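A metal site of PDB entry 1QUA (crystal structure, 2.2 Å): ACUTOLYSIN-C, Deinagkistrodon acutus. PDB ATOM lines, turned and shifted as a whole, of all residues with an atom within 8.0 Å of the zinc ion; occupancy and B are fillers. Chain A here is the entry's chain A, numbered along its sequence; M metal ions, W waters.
Three residues have an atom within 4 Å of the zinc ion: His 141, His 145 and His 151.
The zinc ion is bound by a ring nitrogen (NE2) of His 151 (1.9 Å), water W1 (2.0 Å), a ring nitrogen (NE2) of His 141 (2.1 Å) and a ring nitrogen (NE2) of His 145 (2.1 Å).
The zinc ion has four donor atoms within binding distance.
ND1 of His 145 sits at hydrogen-bond distance from O of Met 149 (2.8 Å).
ND1 of His 141 is in hydrogen-bond range of O of Ile 162 (2.9 Å).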
ATOM      1  N   GLY A 108      16.925   3.201 -23.154  1.00  0.00           N
ATOM      2  CA  GLY A 108      17.018   1.971 -23.917  1.00  0.00           C
ATOM      3  C   GLY A 108      17.511   0.851 -23.002  1.00  0.00           C
ATOM      4  O   GLY A 108      18.035   1.118 -21.910  1.00  0.00           O
ATOM      5  N   LEU A 109      17.364  -0.402 -23.409  1.00  0.00           N
ATOM      6  CA  LEU A 109      17.816  -1.500 -22.562  1.00  0.00           C
ATOM      7  C   LEU A 109      17.860  -2.768 -23.425  1.00  0.00           C
ATOM      8  O   LEU A 109      17.110  -2.884 -24.389  1.00  0.00           O
ATOM      9  CB  LEU A 109      16.848  -1.665 -21.381  1.00  0.00           C
ATOM     10  CG  LEU A 109      17.304  -2.470 -20.143  1.00  0.00           C
ATOM     11  CD1 LEU A 109      18.491  -1.835 -19.504  1.00  0.00           C
ATOM     12  CD2 LEU A 109      16.178  -2.600 -19.146  1.00  0.00           C
ATOM     13  N   ALA A 110      18.805  -3.665 -23.154  1.00  0.00           N
ATOM     14  CA  ALA A 110      18.955  -4.936 -23.882  1.00  0.00           C
ATOM     15  C   ALA A 110      19.524  -5.998 -22.918  1.00  0.00           C
ATOM     16  O   ALA A 110      19.803  -5.679 -21.769  1.00  0.00           O
ATOM     17  CB  ALA A 110      19.881  -4.770 -25.073  1.00  0.00           C
ATOM     18  N   THR A 138      21.674   5.184 -30.160  1.00  0.00           N
ATOM     19  CA  THR A 138      20.964   4.497 -29.090  1.00  0.00           C
ATOM     20  C   THR A 138      20.689   3.057 -29.552  1.00  0.00           C
ATOM     21  O   THR A 138      20.917   2.123 -28.787  1.00  0.00           O
ATOM     22  CB  THR A 138      19.650   5.198 -28.696  1.00  0.00           C
ATOM     23  OG1 THR A 138      19.933   6.529 -28.277  1.00  0.00           O
ATOM     24  CG2 THR A 138      18.992   4.460 -27.541  1.00  0.00           C
ATOM     25  N   HIS A 141      23.813   0.998 -29.636  1.00  0.00           N
ATOM     26  CA  HIS A 141      24.248   0.751 -28.244  1.00  0.00           C
ATOM     27  C   HIS A 141      23.601  -0.501 -27.587  1.00  0.00           C
ATOM     28  O   HIS A 141      24.258  -1.260 -26.868  1.00  0.00           O
ATOM     29  CB  HIS A 141      23.923   1.982 -27.363  1.00  0.00           C
ATOM     30  CG  HIS A 141      24.437   1.885 -25.957  1.00  0.00           C
ATOM     31  ND1 HIS A 141      25.606   2.453 -25.520  1.00  0.00           N
ATOM     32  CD2 HIS A 141      23.870   1.326 -24.865  1.00  0.00           C
ATOM     33  CE1 HIS A 141      25.709   2.242 -24.194  1.00  0.00           C
ATOM     34  NE2 HIS A 141      24.670   1.549 -23.743  1.00  0.00           N
ATOM     35  N   GLU A 142      22.298  -0.661 -27.747  1.00  0.00           N
ATOM     36  CA  GLU A 142      21.623  -1.821 -27.176  1.00  0.00           C
ATOM     37  C   GLU A 142      21.995  -3.064 -27.980  1.00  0.00           C
ATOM     38  O   GLU A 142      22.187  -4.136 -27.407  1.00  0.00           O
ATOM     39  CB  GLU A 142      20.104  -1.612 -27.173  1.00  0.00           C
ATOM     40  CG  GLU A 142      19.670  -0.347 -26.412  1.00  0.00           C
ATOM     41  CD  GLU A 142      20.243  -0.305 -25.027  1.00  0.00           C
ATOM     42  OE1 GLU A 142      20.518  -1.397 -24.471  1.00  0.00           O
ATOM     43  OE2 GLU A 142      20.457   0.804 -24.489  1.00  0.00           O
ATOM     44  N   GLY A 144      24.713  -3.439 -29.359  1.00  0.00           N
ATOM     45  CA  GLY A 144      26.058  -3.724 -28.896  1.00  0.00           C
ATOM     46  C   GLY A 144      26.005  -4.562 -27.630  1.00  0.00           C
ATOM     47  O   GLY A 144      26.856  -5.436 -27.418  1.00  0.00           O
ATOM     48  N   HIS A 145      25.025  -4.332 -26.760  1.00  0.00           N
ATOM     49  CA  HIS A 145      24.887  -5.139 -25.537  1.00  0.00           C
ATOM     50  C   HIS A 145      24.558  -6.640 -25.839  1.00  0.00           C
ATOM     51  O   HIS A 145      25.156  -7.557 -25.252  1.00  0.00           O
ATOM     52  CB  HIS A 145      23.839  -4.518 -24.628  1.00  0.00           C
ATOM     53  CG  HIS A 145      24.337  -3.367 -23.816  1.00  0.00           C
ATOM     54  ND1 HIS A 145      25.557  -3.352 -23.176  1.00  0.00           N
ATOM     55  CD2 HIS A 145      23.721  -2.214 -23.451  1.00  0.00           C
ATOM     56  CE1 HIS A 145      25.620  -2.233 -22.463  1.00  0.00           C
ATOM     57  NE2 HIS A 145      24.503  -1.516 -22.611  1.00  0.00           N
ATOM     58  N   MET A 149      28.806  -6.470 -25.549  1.00  0.00           N
ATOM     59  CA  MET A 149      29.607  -5.316 -25.143  1.00  0.00           C
ATOM     60  C   MET A 149      29.184  -4.699 -23.842  1.00  0.00           C
ATOM     61  O   MET A 149      27.983  -4.588 -23.566  1.00  0.00           O
ATOM     62  CB  MET A 149      29.581  -4.249 -26.214  1.00  0.00           C
ATOM     63  CG  MET A 149      30.303  -4.620 -27.469  1.00  0.00           C
ATOM     64  SD  MET A 149      29.785  -3.543 -28.792  1.00  0.00           S
ATOM     65  CE  MET A 149      30.268  -4.488 -30.242  1.00  0.00           C
ATOM     66  N   ASN A 150      30.162  -4.354 -23.024  1.00  0.00           N
ATOM     67  CA  ASN A 150      29.962  -3.671 -21.740  1.00  0.00           C
ATOM     68  C   ASN A 150      30.144  -2.168 -22.027  1.00  0.00           C
ATOM     69  O   ASN A 150      30.570  -1.768 -23.119  1.00  0.00           O
ATOM     70  CB  ASN A 150      31.055  -4.070 -20.728  1.00  0.00           C
ATOM     71  CG  ASN A 150      30.675  -5.278 -19.881  1.00  0.00           C
ATOM     72  OD1 ASN A 150      31.493  -6.192 -19.685  1.00  0.00           O
ATOM     73  ND2 ASN A 150      29.441  -5.299 -19.389  1.00  0.00           N
ATOM     74  N   HIS A 151      29.900  -1.330 -21.029  1.00  0.00           N
ATOM     75  CA  HIS A 151      30.092   0.090 -21.183  1.00  0.00           C
ATOM     76  C   HIS A 151      31.570   0.390 -21.103  1.00  0.00           C
ATOM     77  O   HIS A 151      32.352  -0.399 -20.543  1.00  0.00           O
ATOM     78  CB  HIS A 151      29.361   0.864 -20.101  1.00  0.00           C
ATOM     79  CG  HIS A 151      27.877   0.825 -20.231  1.00  0.00           C
ATOM     80  ND1 HIS A 151      27.001   1.041 -19.190  1.00  0.00           N
ATOM     81  CD2 HIS A 151      27.098   0.581 -21.319  1.00  0.00           C
ATOM     82  CE1 HIS A 151      25.765   0.904 -19.683  1.00  0.00           C
ATOM     83  NE2 HIS A 151      25.785   0.623 -20.977  1.00  0.00           N
ATOM     84  N   ASP A 152      31.953   1.504 -21.732  1.00  0.00           N
ATOM     85  CA  ASP A 152      33.328   1.967 -21.725  1.00  0.00           C
ATOM     86  C   ASP A 152      33.619   2.562 -20.344  1.00  0.00           C
ATOM     87  O   ASP A 152      32.918   3.465 -19.886  1.00  0.00           O
ATOM     88  CB  ASP A 152      33.553   3.050 -22.786  1.00  0.00           C
ATOM     89  CG  ASP A 152      33.547   2.491 -24.199  1.00  0.00           C
ATOM     90  OD1 ASP A 152      33.963   1.338 -24.373  1.00  0.00           O
ATOM     91  OD2 ASP A 152      33.132   3.220 -25.136  1.00  0.00           O
ATOM     92  N   ILE A 162      30.481   4.533 -29.066  1.00  0.00           N
ATOM     93  CA  ILE A 162      29.146   3.960 -29.005  1.00  0.00           C
ATOM     94  C   ILE A 162      28.722   3.454 -27.601  1.00  0.00           C
ATOM     95  O   ILE A 162      27.635   3.781 -27.120  1.00  0.00           O
ATOM     96  CB  ILE A 162      28.985   2.818 -30.092  1.00  0.00           C
ATOM     97  CG1 ILE A 162      29.234   3.375 -31.495  1.00  0.00           C
ATOM     98  CG2 ILE A 162      27.588   2.215 -30.076  1.00  0.00           C
ATOM     99  CD1 ILE A 162      28.086   4.218 -31.983  1.00  0.00           C
ATOM    100  N   MET A 163      29.622   2.722 -26.923  1.00  0.00           N
ATOM    101  CA  MET A 163      29.305   2.137 -25.632  1.00  0.00           C
ATOM    102  C   MET A 163      29.523   3.006 -24.411  1.00  0.00           C
ATOM    103  O   MET A 163      29.563   2.518 -23.264  1.00  0.00           O
ATOM    104  CB  MET A 163      29.996   0.776 -25.486  1.00  0.00           C
ATOM    105  CG  MET A 163      29.639  -0.234 -26.568  1.00  0.00           C
ATOM    106  SD  MET A 163      27.861  -0.538 -26.758  1.00  0.00           S
ATOM    107  CE  MET A 163      27.337  -0.964 -25.210  1.00  0.00           C
ATOM    108  N   ALA A 164      29.618   4.309 -24.649  1.00  0.00           N
ATOM    109  CA  ALA A 164      29.761   5.230 -23.533  1.00  0.00           C
ATOM    110  C   ALA A 164      28.485   5.005 -22.705  1.00  0.00           C
ATOM    111  O   ALA A 164      27.395   4.807 -23.264  1.00  0.00           O
ATOM    112  CB  ALA A 164      29.840   6.677 -24.029  1.00  0.00           C
ATOM    113  N   PRO A 165      28.605   5.043 -21.372  1.00  0.00           N
ATOM    114  CA  PRO A 165      27.510   4.843 -20.419  1.00  0.00           C
ATOM    115  C   PRO A 165      26.307   5.760 -20.498  1.00  0.00           C
ATOM    116  O   PRO A 165      25.204   5.339 -20.154  1.00  0.00           O
ATOM    117  CB  PRO A 165      28.201   4.914 -19.070  1.00  0.00           C
ATOM    118  CG  PRO A 165      29.337   5.794 -19.343  1.00  0.00           C
ATOM    119  CD  PRO A 165      29.851   5.377 -20.671  1.00  0.00           C
ATOM    120  N   VAL A 166      26.525   7.023 -20.860  1.00  0.00           N
ATOM    121  CA  VAL A 166      25.418   7.980 -21.031  1.00  0.00           C
ATOM    122  C   VAL A 166      25.612   8.688 -22.373  1.00  0.00           C
ATOM    123  O   VAL A 166      26.731   8.820 -22.863  1.00  0.00           O
ATOM    124  CB  VAL A 166      25.299   9.015 -19.906  1.00  0.00           C
ATOM    125  CG1 VAL A 166      24.605   8.395 -18.655  1.00  0.00           C
ATOM    126  CG2 VAL A 166      26.661   9.593 -19.573  1.00  0.00           C
HETATM  127 ZN    ZN M   1      24.254   0.459 -22.052  1.00  0.00          ZN
HETATM  128  O   HOH W   1      22.331   0.506 -21.538  1.00  0.00           O
